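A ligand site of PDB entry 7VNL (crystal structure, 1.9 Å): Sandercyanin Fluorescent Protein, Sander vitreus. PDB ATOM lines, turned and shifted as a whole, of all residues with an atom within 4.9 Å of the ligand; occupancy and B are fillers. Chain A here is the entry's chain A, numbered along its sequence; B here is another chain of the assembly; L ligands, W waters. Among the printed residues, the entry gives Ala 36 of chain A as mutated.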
ATOM      1  N   TRP A  26      26.062  29.332  -5.964  1.00  0.00           N
ATOM      2  CA  TRP A  26      26.917  28.250  -6.406  1.00  0.00           C
ATOM      3  C   TRP A  26      26.177  26.919  -6.250  1.00  0.00           C
ATOM      4  O   TRP A  26      25.533  26.697  -5.220  1.00  0.00           O
ATOM      5  CB  TRP A  26      28.207  28.212  -5.570  1.00  0.00           C
ATOM      6  CG  TRP A  26      29.157  29.357  -5.854  1.00  0.00           C
ATOM      7  CD1 TRP A  26      29.381  30.483  -5.084  1.00  0.00           C
ATOM      8  CD2 TRP A  26      30.056  29.441  -6.948  1.00  0.00           C
ATOM      9  NE1 TRP A  26      30.361  31.267  -5.674  1.00  0.00           N
ATOM     10  CE2 TRP A  26      30.786  30.642  -6.819  1.00  0.00           C
ATOM     11  CE3 TRP A  26      30.311  28.607  -8.046  1.00  0.00           C
ATOM     12  CZ2 TRP A  26      31.760  31.033  -7.740  1.00  0.00           C
ATOM     13  CZ3 TRP A  26      31.269  28.987  -8.951  1.00  0.00           C
ATOM     14  CH2 TRP A  26      31.982  30.200  -8.799  1.00  0.00           C
ATOM     15  N   TYR A  27      26.284  26.047  -7.253  1.00  0.00           N
ATOM     16  CA  TYR A  27      25.658  24.730  -7.237  1.00  0.00           C
ATOM     17  C   TYR A  27      26.691  23.675  -6.905  1.00  0.00           C
ATOM     18  O   TYR A  27      27.771  23.657  -7.500  1.00  0.00           O
ATOM     19  CB  TYR A  27      25.025  24.392  -8.598  1.00  0.00           C
ATOM     20  CG  TYR A  27      23.835  25.268  -8.914  1.00  0.00           C
ATOM     21  CD1 TYR A  27      24.009  26.503  -9.537  1.00  0.00           C
ATOM     22  CD2 TYR A  27      22.536  24.859  -8.615  1.00  0.00           C
ATOM     23  CE1 TYR A  27      22.924  27.320  -9.826  1.00  0.00           C
ATOM     24  CE2 TYR A  27      21.439  25.672  -8.908  1.00  0.00           C
ATOM     25  CZ  TYR A  27      21.656  26.904  -9.515  1.00  0.00           C
ATOM     26  OH  TYR A  27      20.609  27.732  -9.817  1.00  0.00           O
ATOM     27  N   ASP A  28      26.338  22.765  -6.009  1.00  0.00           N
ATOM     28  CA  ASP A  28      27.197  21.640  -5.680  1.00  0.00           C
ATOM     29  C   ASP A  28      27.217  20.629  -6.825  1.00  0.00           C
ATOM     30  O   ASP A  28      26.160  20.121  -7.216  1.00  0.00           O
ATOM     31  CB  ASP A  28      26.704  20.991  -4.388  1.00  0.00           C
ATOM     32  CG  ASP A  28      27.738  20.076  -3.787  1.00  0.00           C
ATOM     33  OD1 ASP A  28      28.688  20.579  -3.137  1.00  0.00           O
ATOM     34  OD2 ASP A  28      27.603  18.857  -3.971  1.00  0.00           O
ATOM     35  N   ALA A  36      27.189  16.516   7.096  1.00  0.00           N
ATOM     36  CA  ALA A  36      26.451  17.805   6.954  1.00  0.00           C
ATOM     37  C   ALA A  36      25.322  17.769   5.912  1.00  0.00           C
ATOM     38  O   ALA A  36      24.213  18.193   6.244  1.00  0.00           O
ATOM     39  CB  ALA A  36      27.447  18.906   6.640  1.00  0.00           C
ATOM     40  N   GLN A  37      25.620  17.352   4.681  1.00  0.00           N
ATOM     41  CA  GLN A  37      24.643  17.315   3.553  1.00  0.00           C
ATOM     42  C   GLN A  37      24.018  15.934   3.400  1.00  0.00           C
ATOM     43  O   GLN A  37      24.673  15.045   2.846  1.00  0.00           O
ATOM     44  CB  GLN A  37      25.342  17.718   2.261  1.00  0.00           C
ATOM     45  CG  GLN A  37      25.854  19.146   2.244  1.00  0.00           C
ATOM     46  CD  GLN A  37      26.646  19.413   0.984  1.00  0.00           C
ATOM     47  OE1 GLN A  37      26.082  19.563  -0.092  1.00  0.00           O
ATOM     48  NE2 GLN A  37      27.954  19.487   1.117  1.00  0.00           N
ATOM     49  N   ALA A  42      22.080  20.713  -3.786  1.00  0.00           N
ATOM     50  CA  ALA A  42      22.614  21.696  -2.864  1.00  0.00           C
ATOM     51  C   ALA A  42      23.093  22.954  -3.576  1.00  0.00           C
ATOM     52  O   ALA A  42      23.737  22.886  -4.638  1.00  0.00           O
ATOM     53  CB  ALA A  42      23.758  21.092  -2.051  1.00  0.00           C
ATOM     54  N   THR A  43      22.776  24.106  -2.987  1.00  0.00           N
ATOM     55  CA  THR A  43      23.318  25.396  -3.405  1.00  0.00           C
ATOM     56  C   THR A  43      23.839  26.144  -2.189  1.00  0.00           C
ATOM     57  O   THR A  43      23.353  25.953  -1.065  1.00  0.00           O
ATOM     58  CB  THR A  43      22.266  26.272  -4.095  1.00  0.00           C
ATOM     59  OG1 THR A  43      21.270  26.610  -3.130  1.00  0.00           O
ATOM     60  CG2 THR A  43      21.618  25.557  -5.274  1.00  0.00           C
ATOM     61  N   ALA A  44      24.814  27.003  -2.426  1.00  0.00           N
ATOM     62  CA  ALA A  44      25.314  27.956  -1.444  1.00  0.00           C
ATOM     63  C   ALA A  44      25.097  29.345  -2.004  1.00  0.00           C
ATOM     64  O   ALA A  44      25.412  29.596  -3.174  1.00  0.00           O
ATOM     65  CB  ALA A  44      26.796  27.705  -1.129  1.00  0.00           C
ATOM     66  N   TYR A  46      26.049  33.328  -1.221  1.00  0.00           N
ATOM     67  CA  TYR A  46      26.914  34.224  -0.464  1.00  0.00           C
ATOM     68  C   TYR A  46      26.469  35.654  -0.712  1.00  0.00           C
ATOM     69  O   TYR A  46      26.268  36.051  -1.860  1.00  0.00           O
ATOM     70  CB  TYR A  46      28.369  34.010  -0.872  1.00  0.00           C
ATOM     71  CG  TYR A  46      28.810  32.572  -0.690  1.00  0.00           C
ATOM     72  CD1 TYR A  46      28.473  31.859   0.464  1.00  0.00           C
ATOM     73  CD2 TYR A  46      29.539  31.912  -1.679  1.00  0.00           C
ATOM     74  CE1 TYR A  46      28.877  30.511   0.638  1.00  0.00           C
ATOM     75  CE2 TYR A  46      29.933  30.590  -1.530  1.00  0.00           C
ATOM     76  CZ  TYR A  46      29.604  29.894  -0.370  1.00  0.00           C
ATOM     77  OH  TYR A  46      30.016  28.589  -0.254  1.00  0.00           O
ATOM     78  N   ASN A  58      22.978  28.227   2.833  1.00  0.00           N
ATOM     79  CA  ASN A  58      23.043  26.959   2.118  1.00  0.00           C
ATOM     80  C   ASN A  58      21.674  26.307   2.106  1.00  0.00           C
ATOM     81  O   ASN A  58      20.961  26.321   3.119  1.00  0.00           O
ATOM     82  CB  ASN A  58      24.033  25.993   2.782  1.00  0.00           C
ATOM     83  CG  ASN A  58      25.452  26.513   2.779  1.00  0.00           C
ATOM     84  OD1 ASN A  58      25.832  27.335   1.953  1.00  0.00           O
ATOM     85  ND2 ASN A  58      26.266  26.024   3.712  1.00  0.00           N
ATOM     86  N   ARG A  59      21.306  25.700   0.978  1.00  0.00           N
ATOM     87  CA  ARG A  59      20.022  25.047   0.807  1.00  0.00           C
ATOM     88  C   ARG A  59      20.231  23.681   0.175  1.00  0.00           C
ATOM     89  O   ARG A  59      21.085  23.514  -0.700  1.00  0.00           O
ATOM     90  CB  ARG A  59      19.065  25.850  -0.107  1.00  0.00           C
ATOM     91  CG  ARG A  59      18.828  27.281   0.330  1.00  0.00           C
ATOM     92  CD  ARG A  59      18.140  28.080  -0.772  1.00  0.00           C
ATOM     93  NE  ARG A  59      16.732  27.735  -0.869  1.00  0.00           N
ATOM     94  CZ  ARG A  59      16.087  27.436  -1.986  1.00  0.00           C
ATOM     95  NH1 ARG A  59      16.696  27.465  -3.168  1.00  0.00           N
ATOM     96  NH2 ARG A  59      14.807  27.100  -1.926  1.00  0.00           N
ATOM     97  N   GLU A  60      19.410  22.722   0.580  1.00  0.00           N
ATOM     98  CA  GLU A  60      19.408  21.452  -0.112  1.00  0.00           C
ATOM     99  C   GLU A  60      18.003  20.863  -0.066  1.00  0.00           C
ATOM    100  O   GLU A  60      17.152  21.284   0.723  1.00  0.00           O
ATOM    101  CB  GLU A  60      20.445  20.494   0.475  1.00  0.00           C
ATOM    102  CG  GLU A  60      20.102  20.001   1.881  1.00  0.00           C
ATOM    103  CD  GLU A  60      21.035  18.892   2.351  1.00  0.00           C
ATOM    104  OE1 GLU A  60      21.717  18.267   1.505  1.00  0.00           O
ATOM    105  OE2 GLU A  60      21.056  18.630   3.573  1.00  0.00           O
ATOM    106  N   LYS A  68      15.941  21.989   3.338  1.00  0.00           N
ATOM    107  CA  LYS A  68      16.672  22.306   4.546  1.00  0.00           C
ATOM    108  C   LYS A  68      17.681  23.386   4.238  1.00  0.00           C
ATOM    109  O   LYS A  68      18.350  23.348   3.190  1.00  0.00           O
ATOM    110  CB  LYS A  68      17.381  21.083   5.120  1.00  0.00           C
ATOM    111  CG  LYS A  68      18.233  21.425   6.331  1.00  0.00           C
ATOM    112  CD  LYS A  68      17.632  21.043   7.664  1.00  0.00           C
ATOM    113  CE  LYS A  68      18.760  20.834   8.678  1.00  0.00           C
ATOM    114  NZ  LYS A  68      19.297  19.448   8.645  1.00  0.00           N
ATOM    115  N   VAL A  70      20.690  26.301   6.046  1.00  0.00           N
ATOM    116  CA  VAL A  70      21.501  26.701   7.186  1.00  0.00           C
ATOM    117  C   VAL A  70      22.096  28.079   6.899  1.00  0.00           C
ATOM    118  O   VAL A  70      22.442  28.399   5.756  1.00  0.00           O
ATOM    119  CB  VAL A  70      22.594  25.657   7.508  1.00  0.00           C
ATOM    120  CG1 VAL A  70      23.631  25.562   6.384  1.00  0.00           C
ATOM    121  CG2 VAL A  70      23.269  25.991   8.830  1.00  0.00           C
ATOM    122  N   PHE A  87      34.346  29.557   8.355  1.00  0.00           N
ATOM    123  CA  PHE A  87      32.893  29.548   8.256  1.00  0.00           C
ATOM    124  C   PHE A  87      32.299  29.231   9.622  1.00  0.00           C
ATOM    125  O   PHE A  87      32.695  28.263  10.269  1.00  0.00           O
ATOM    126  CB  PHE A  87      32.383  28.524   7.227  1.00  0.00           C
ATOM    127  CG  PHE A  87      32.278  29.070   5.823  1.00  0.00           C
ATOM    128  CD1 PHE A  87      33.255  29.916   5.317  1.00  0.00           C
ATOM    129  CD2 PHE A  87      31.199  28.722   5.015  1.00  0.00           C
ATOM    130  CE1 PHE A  87      33.166  30.397   3.999  1.00  0.00           C
ATOM    131  CE2 PHE A  87      31.085  29.221   3.710  1.00  0.00           C
ATOM    132  CZ  PHE A  87      32.071  30.063   3.204  1.00  0.00           C
ATOM    133  N   HIS A  89      28.759  28.409  11.101  1.00  0.00           N
ATOM    134  CA  HIS A  89      27.360  28.062  10.877  1.00  0.00           C
ATOM    135  C   HIS A  89      26.628  27.975  12.204  1.00  0.00           C
ATOM    136  O   HIS A  89      27.208  27.645  13.244  1.00  0.00           O
ATOM    137  CB  HIS A  89      27.211  26.710  10.149  1.00  0.00           C
ATOM    138  CG  HIS A  89      27.989  26.581   8.874  1.00  0.00           C
ATOM    139  ND1 HIS A  89      29.321  26.252   8.847  1.00  0.00           N
ATOM    140  CD2 HIS A  89      27.591  26.691   7.585  1.00  0.00           C
ATOM    141  CE1 HIS A  89      29.726  26.170   7.590  1.00  0.00           C
ATOM    142  NE2 HIS A  89      28.700  26.428   6.807  1.00  0.00           N
ATOM    143  N   GLU A  90      25.336  28.273  12.174  1.00  0.00           N
ATOM    144  CA  GLU A  90      24.546  28.086  13.376  1.00  0.00           C
ATOM    145  C   GLU A  90      24.632  26.631  13.812  1.00  0.00           C
ATOM    146  O   GLU A  90      24.585  25.728  12.980  1.00  0.00           O
ATOM    147  CB  GLU A  90      23.106  28.574  13.122  1.00  0.00           C
ATOM    148  CG  GLU A  90      22.308  27.713  12.163  1.00  0.00           C
ATOM    149  CD  GLU A  90      21.016  28.392  11.662  1.00  0.00           C
ATOM    150  OE1 GLU A  90      20.548  28.049  10.544  1.00  0.00           O
ATOM    151  OE2 GLU A  90      20.422  29.215  12.436  1.00  0.00           O
ATOM    152  N   ASN A  91      24.915  26.413  15.093  1.00  0.00           N
ATOM    153  CA  ASN A  91      25.046  25.076  15.681  1.00  0.00           C
ATOM    154  C   ASN A  91      26.316  24.331  15.265  1.00  0.00           C
ATOM    155  O   ASN A  91      26.419  23.115  15.485  1.00  0.00           O
ATOM    156  CB  ASN A  91      23.836  24.205  15.352  1.00  0.00           C
ATOM    157  CG  ASN A  91      22.654  24.521  16.232  1.00  0.00           C
ATOM    158  OD1 ASN A  91      21.682  25.131  15.773  1.00  0.00           O
ATOM    159  ND2 ASN A  91      22.718  24.086  17.488  1.00  0.00           N
ATOM    160  N   ALA A  92      27.300  25.001  14.692  1.00  0.00           N
ATOM    161  CA  ALA A  92      28.554  24.338  14.355  1.00  0.00           C
ATOM    162  C   ALA A  92      29.729  25.073  14.984  1.00  0.00           C
ATOM    163  O   ALA A  92      29.717  26.309  15.090  1.00  0.00           O
ATOM    164  CB  ALA A  92      28.759  24.236  12.842  1.00  0.00           C
ATOM    165  N   VAL A  95      34.773  26.078  11.112  1.00  0.00           N
ATOM    166  CA  VAL A  95      35.482  25.200  10.166  1.00  0.00           C
ATOM    167  C   VAL A  95      36.214  26.032   9.113  1.00  0.00           C
ATOM    168  O   VAL A  95      35.708  27.090   8.693  1.00  0.00           O
ATOM    169  CB  VAL A  95      34.521  24.210   9.492  1.00  0.00           C
ATOM    170  CG1 VAL A  95      33.790  23.330  10.549  1.00  0.00           C
ATOM    171  CG2 VAL A  95      33.525  24.950   8.637  1.00  0.00           C
ATOM    172  N   PRO A  96      37.369  25.593   8.645  1.00  0.00           N
ATOM    173  CA  PRO A  96      38.052  26.318   7.563  1.00  0.00           C
ATOM    174  C   PRO A  96      37.290  26.180   6.261  1.00  0.00           C
ATOM    175  O   PRO A  96      36.506  25.250   6.065  1.00  0.00           O
ATOM    176  CB  PRO A  96      39.440  25.677   7.462  1.00  0.00           C
ATOM    177  CG  PRO A  96      39.419  24.456   8.353  1.00  0.00           C
ATOM    178  CD  PRO A  96      38.136  24.429   9.150  1.00  0.00           C
ATOM    179  N   TYR A  97      37.503  27.146   5.354  1.00  0.00           N
ATOM    180  CA  TYR A  97      36.925  27.102   4.012  1.00  0.00           C
ATOM    181  C   TYR A  97      37.942  27.782   3.106  1.00  0.00           C
ATOM    182  O   TYR A  97      38.139  28.995   3.233  1.00  0.00           O
ATOM    183  CB  TYR A  97      35.560  27.798   3.974  1.00  0.00           C
ATOM    184  CG  TYR A  97      34.782  27.918   2.659  1.00  0.00           C
ATOM    185  CD1 TYR A  97      35.208  28.751   1.631  1.00  0.00           C
ATOM    186  CD2 TYR A  97      33.571  27.232   2.486  1.00  0.00           C
ATOM    187  CE1 TYR A  97      34.462  28.888   0.442  1.00  0.00           C
ATOM    188  CE2 TYR A  97      32.809  27.383   1.311  1.00  0.00           C
ATOM    189  CZ  TYR A  97      33.265  28.210   0.295  1.00  0.00           C
ATOM    190  OH  TYR A  97      32.516  28.340  -0.875  1.00  0.00           O
ATOM    191  N   VAL A 110      36.646  24.087  -3.577  1.00  0.00           N
ATOM    192  CA  VAL A 110      36.699  24.498  -2.173  1.00  0.00           C
ATOM    193  C   VAL A 110      37.158  23.321  -1.331  1.00  0.00           C
ATOM    194  O   VAL A 110      36.821  22.170  -1.636  1.00  0.00           O
ATOM    195  CB  VAL A 110      35.327  25.039  -1.711  1.00  0.00           C
ATOM    196  CG1 VAL A 110      35.337  25.377  -0.220  1.00  0.00           C
ATOM    197  CG2 VAL A 110      35.013  26.316  -2.501  1.00  0.00           C
ATOM    198  N   TYR A 111      37.940  23.608  -0.286  1.00  0.00           N
ATOM    199  CA  TYR A 111      38.572  22.575   0.520  1.00  0.00           C
ATOM    200  C   TYR A 111      38.522  22.997   1.988  1.00  0.00           C
ATOM    201  O   TYR A 111      38.690  24.188   2.294  1.00  0.00           O
ATOM    202  CB  TYR A 111      40.028  22.340   0.074  1.00  0.00           C
ATOM    203  CG  TYR A 111      40.700  21.201   0.808  1.00  0.00           C
ATOM    204  CD1 TYR A 111      40.263  19.896   0.630  1.00  0.00           C
ATOM    205  CD2 TYR A 111      41.732  21.440   1.712  1.00  0.00           C
ATOM    206  CE1 TYR A 111      40.864  18.845   1.310  1.00  0.00           C
ATOM    207  CE2 TYR A 111      42.336  20.395   2.404  1.00  0.00           C
ATOM    208  CZ  TYR A 111      41.893  19.103   2.198  1.00  0.00           C
ATOM    209  OH  TYR A 111      42.486  18.059   2.868  1.00  0.00           O
ATOM    210  N   SER A 112      38.302  22.041   2.876  1.00  0.00           N
ATOM    211  CA  SER A 112      38.263  22.295   4.312  1.00  0.00           C
ATOM    212  C   SER A 112      38.871  21.113   5.023  1.00  0.00           C
ATOM    213  O   SER A 112      38.447  19.986   4.789  1.00  0.00           O
ATOM    214  CB  SER A 112      36.830  22.506   4.796  1.00  0.00           C
ATOM    215  OG  SER A 112      36.781  22.716   6.205  1.00  0.00           O
ATOM    216  N   TYR A 123      36.363  18.307   4.059  1.00  0.00           N
ATOM    217  CA  TYR A 123      35.373  18.482   2.999  1.00  0.00           C
ATOM    218  C   TYR A 123      36.075  18.963   1.744  1.00  0.00           C
ATOM    219  O   TYR A 123      37.068  19.704   1.821  1.00  0.00           O
ATOM    220  CB  TYR A 123      34.297  19.541   3.278  1.00  0.00           C
ATOM    221  CG  TYR A 123      33.486  19.501   4.547  1.00  0.00           C
ATOM    222  CD1 TYR A 123      32.153  19.100   4.536  1.00  0.00           C
ATOM    223  CD2 TYR A 123      33.986  20.059   5.708  1.00  0.00           C
ATOM    224  CE1 TYR A 123      31.393  19.126   5.696  1.00  0.00           C
ATOM    225  CE2 TYR A 123      33.221  20.100   6.861  1.00  0.00           C
ATOM    226  CZ  TYR A 123      31.922  19.628   6.842  1.00  0.00           C
ATOM    227  OH  TYR A 123      31.172  19.678   7.989  1.00  0.00           O
ATOM    228  N   ALA A 124      35.530  18.620   0.594  1.00  0.00           N
ATOM    229  CA  ALA A 124      36.016  19.157  -0.671  1.00  0.00           C
ATOM    230  C   ALA A 124      34.844  19.194  -1.641  1.00  0.00           C
ATOM    231  O   ALA A 124      34.085  18.219  -1.722  1.00  0.00           O
ATOM    232  CB  ALA A 124      37.169  18.329  -1.246  1.00  0.00           C
ATOM    233  N   SER A 125      34.706  20.301  -2.379  1.00  0.00           N
ATOM    234  CA  SER A 125      33.572  20.444  -3.278  1.00  0.00           C
ATOM    235  C   SER A 125      33.993  21.105  -4.575  1.00  0.00           C
ATOM    236  O   SER A 125      34.720  22.109  -4.564  1.00  0.00           O
ATOM    237  CB  SER A 125      32.470  21.261  -2.615  1.00  0.00           C
ATOM    238  OG  SER A 125      31.254  21.070  -3.305  1.00  0.00           O
ATOM    239  N   VAL A 127      32.080  23.210  -7.331  1.00  0.00           N
ATOM    240  CA  VAL A 127      30.826  23.938  -7.492  1.00  0.00           C
ATOM    241  C   VAL A 127      30.850  24.694  -8.811  1.00  0.00           C
ATOM    242  O   VAL A 127      31.904  24.910  -9.406  1.00  0.00           O
ATOM    243  CB  VAL A 127      30.537  24.913  -6.331  1.00  0.00           C
ATOM    244  CG1 VAL A 127      30.405  24.136  -5.012  1.00  0.00           C
ATOM    245  CG2 VAL A 127      31.640  25.944  -6.229  1.00  0.00           C
ATOM    246  N   GLY B 117      32.865  20.856  12.968  1.00  0.00           N
ATOM    247  CA  GLY B 117      31.649  21.530  12.540  1.00  0.00           C
ATOM    248  C   GLY B 117      30.521  21.234  13.492  1.00  0.00           C
ATOM    249  O   GLY B 117      30.592  21.571  14.673  1.00  0.00           O
ATOM    250  N   ALA B 118      29.442  20.609  13.007  1.00  0.00           N
ATOM    251  CA  ALA B 118      28.351  20.203  13.865  1.00  0.00           C
ATOM    252  C   ALA B 118      28.561  18.800  14.441  1.00  0.00           C
ATOM    253  O   ALA B 118      27.726  18.332  15.217  1.00  0.00           O
ATOM    254  CB  ALA B 118      27.014  20.258  13.102  1.00  0.00           C
HETATM  255  C1  LIG L   1      25.850  22.511   6.166  1.00  0.00           C
HETATM  256  N1  LIG L   1      28.362  22.814   5.855  1.00  0.00           N
HETATM  257  C2  LIG L   1      27.281  22.651   6.645  1.00  0.00           C
HETATM  258  C3  LIG L   1      27.696  22.626   7.965  1.00  0.00           C
HETATM  259  C4  LIG L   1      29.034  22.772   7.967  1.00  0.00           C
HETATM  260  C5  LIG L   1      29.442  22.894   6.661  1.00  0.00           C
HETATM  261  C6  LIG L   1      29.939  22.816   9.193  1.00  0.00           C
HETATM  262  C7  LIG L   1      26.809  22.441   9.187  1.00  0.00           C
HETATM  263  C8  LIG L   1      25.832  23.579   9.387  1.00  0.00           C
HETATM  264  C9  LIG L   1      24.858  23.133  10.481  1.00  0.00           C
HETATM  265  O1  LIG L   1      23.851  22.441  10.174  1.00  0.00           O
HETATM  266  O2  LIG L   1      25.074  23.450  11.695  1.00  0.00           O
HETATM  267  C10 LIG L   1      30.861  23.113   6.199  1.00  0.00           C
HETATM  268  N2  LIG L   1      30.488  22.097   3.876  1.00  0.00           N
HETATM  269  C11 LIG L   1      31.238  22.873   4.961  1.00  0.00           C
HETATM  270  C12 LIG L   1      32.508  23.325   4.344  1.00  0.00           C
HETATM  271  C13 LIG L   1      32.582  22.877   3.008  1.00  0.00           C
HETATM  272  C14 LIG L   1      31.359  22.100   2.635  1.00  0.00           C
HETATM  273  C15 LIG L   1      33.554  24.161   5.074  1.00  0.00           C
HETATM  274  O3  LIG L   1      31.096  21.575   1.591  1.00  0.00           O
HETATM  275  C16 LIG L   1      33.761  23.164   2.081  1.00  0.00           C
HETATM  276  C17 LIG L   1      33.940  22.431   0.995  1.00  0.00           C
HETATM  277  N3  LIG L   1      28.273  23.893   1.944  1.00  0.00           N
HETATM  278  C18 LIG L   1      29.522  24.446   1.272  1.00  0.00           C
HETATM  279  C19 LIG L   1      29.274  24.336  -0.196  1.00  0.00           C
HETATM  280  C20 LIG L   1      27.975  23.774  -0.435  1.00  0.00           C
HETATM  281  C21 LIG L   1      27.311  23.473   0.852  1.00  0.00           C
HETATM  282  C22 LIG L   1      30.294  24.808  -1.233  1.00  0.00           C
HETATM  283  O4  LIG L   1      30.476  24.865   1.833  1.00  0.00           O
HETATM  284  C23 LIG L   1      27.316  23.476  -1.776  1.00  0.00           C
HETATM  285  C24 LIG L   1      26.973  24.448  -2.617  1.00  0.00           C
HETATM  286  C25 LIG L   1      26.128  22.934   1.050  1.00  0.00           C
HETATM  287  N4  LIG L   1      26.474  22.787   3.698  1.00  0.00           N
HETATM  288  C26 LIG L   1      25.646  22.767   2.469  1.00  0.00           C
HETATM  289  C27 LIG L   1      24.227  22.550   2.836  1.00  0.00           C
HETATM  290  C28 LIG L   1      24.164  22.461   4.283  1.00  0.00           C
HETATM  291  C29 LIG L   1      25.557  22.585   4.879  1.00  0.00           C
HETATM  292  C30 LIG L   1      23.059  22.475   1.851  1.00  0.00           C
HETATM  293  C31 LIG L   1      22.927  22.218   5.133  1.00  0.00           C
HETATM  294  C32 LIG L   1      22.952  20.709   5.299  1.00  0.00           C
HETATM  295  C33 LIG L   1      22.021  20.309   6.434  1.00  0.00           C
HETATM  296  O5  LIG L   1      20.861  19.936   6.117  1.00  0.00           O
HETATM  297  O6  LIG L   1      22.433  20.354   7.638  1.00  0.00           O
HETATM  298  O   HOH W   1      28.533  20.419   3.683  1.00  0.00           O
HETATM  299  O   HOH W   2      28.622  27.495   1.833  1.00  0.00           O
HETATM  300  O   HOH W   3      29.021  25.648   4.113  1.00  0.00           O
HETATM  301  O   HOH W   4      23.528  20.472  11.936  1.00  0.00           O
HETATM  302  O   HOH W   5      31.478  19.419   0.448  1.00  0.00           O
HETATM  303  O   HOH W   6      27.859  19.921  10.091  1.00  0.00           O
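The backbone carbonyl oxygen of Asn 58 lies within hydrogen-bond range of the backbone NH of Val 70, 2.9 Å away. O of Pro 96 sits at hydrogen-bond distance from OG of Ser 112, 2.6 Å away. The backbone NH (N) of Trp 26 sits at hydrogen-bond distance from the backbone carbonyl oxygen (O) of Ala 44 (2.9 Å). The backbone NH (N) of Arg 59 lies within hydrogen-bond range of the backbone carbonyl oxygen (O) of Thr 43 (2.9 Å). The side-chain hydroxyl of Tyr 97 is in hydrogen-bond range of the side-chain hydroxyl of Tyr 46, at 2.6 Å. The backbone NH (N) of Ser 125 sits at hydrogen-bond distance from the backbone carbonyl oxygen (O) of Val 110 (2.9 Å). O of Ala 42 lies within hydrogen-bond range of N of Asp 28, at 2.9 Å. N of Tyr 123 sits at hydrogen-bond distance from O of Ser 112 (2.8 Å).
Water W1 bridges a nitrogen (N2) of the ligand and the side-chain amide nitrogen of Gln 37. Water W3 lies within hydrogen-bond range of ND2 of Asn 58 (2.8 Å), O4 of the ligand (2.8 Å) and NE2 of His 89 (2.8 Å). Water W2 lies within hydrogen-bond range of the side-chain hydroxyl (OH) of Tyr 46 (2.7 Å), the side-chain amide oxygen (OD1) of Asn 58 (2.8 Å) and an oxygen (O4) of the ligand (3.2 Å).
O of Ala 36 lies close to O6 of the ligand, at 3.1 Å. O of Trp 26 touches C24 of the ligand (3.7 Å). Asp 28 touches the ligand (OD1 to C23, 3.5 Å). OE1 of Gln 37 touches C25 of the ligand (3.6 Å). Thr 43 touches the ligand (C to C24, 3.6 Å). Ala 44 touches the ligand. Tyr 46 touches the ligand. O of Arg 59 touches C30 of the ligand, at 3.4 Å. Val 70 touches the ligand (CG2 to C8, 3.6 Å). His 89 touches the ligand. Asn 91 touches the ligand (C to O2, 3.9 Å). Ala 92 touches the ligand (CB to O2, 3.9 Å). CG2 of Val 95 touches C15 of the ligand, at 3.6 Å. Pro 96 touches the ligand (O to C15, 3.3 Å). Tyr 97 touches the ligand (CE2 to O4, 3.5 Å). CG1 of Val 110 touches C17 of the ligand (3.5 Å). Ser 112 touches the ligand (CB to C15, 3.7 Å). Tyr 123 touches the ligand (CD1 to N2, 3.5 Å). Val 127 touches the ligand (CG1 to C22, 3.8 Å). CA of Gly 117 of chain B touches C6 of the ligand, at 3.97 Å. Ala 118 of chain B touches the ligand (CB to O2, 3.99 Å). Hydrophobic or aromatic side chains that line the ligand: Ala 36, Ala 44, Val 70, His 89, Ala 92, Val 95, Tyr 97, Val 110, Tyr 123, Val 127 and Ala 118 of chain B. Within 4 Å of the ligand: Trp 26, Asp 28, Ala 36, Gln 37, Thr 43, Ala 44, Tyr 46, Asn 58, Arg 59, Glu 60, Lys 68, Val 70, His 89, Glu 90, Asn 91, Ala 92, Val 95, Pro 96, Tyr 97, Val 110, Ser 112, Tyr 123, Val 127, Gly 117 of chain B and Ala 118 of chain B. Along chain A the residues within 4 Å of the ligand span positions 26 to 127.
O of Glu 90 sits close to O2 of the ligand, at 2.7 Å. An oxygen (O5) of the ligand lies close to the side-chain carboxylate (OE2) of Glu 60. NZ of Lys 68 lies within salt-bridge range of O5 of the ligand, at 3.0 Å. N4 of the ligand sits at hydrogen-bond distance from ND2 of Asn 58, 3.2 Å away.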
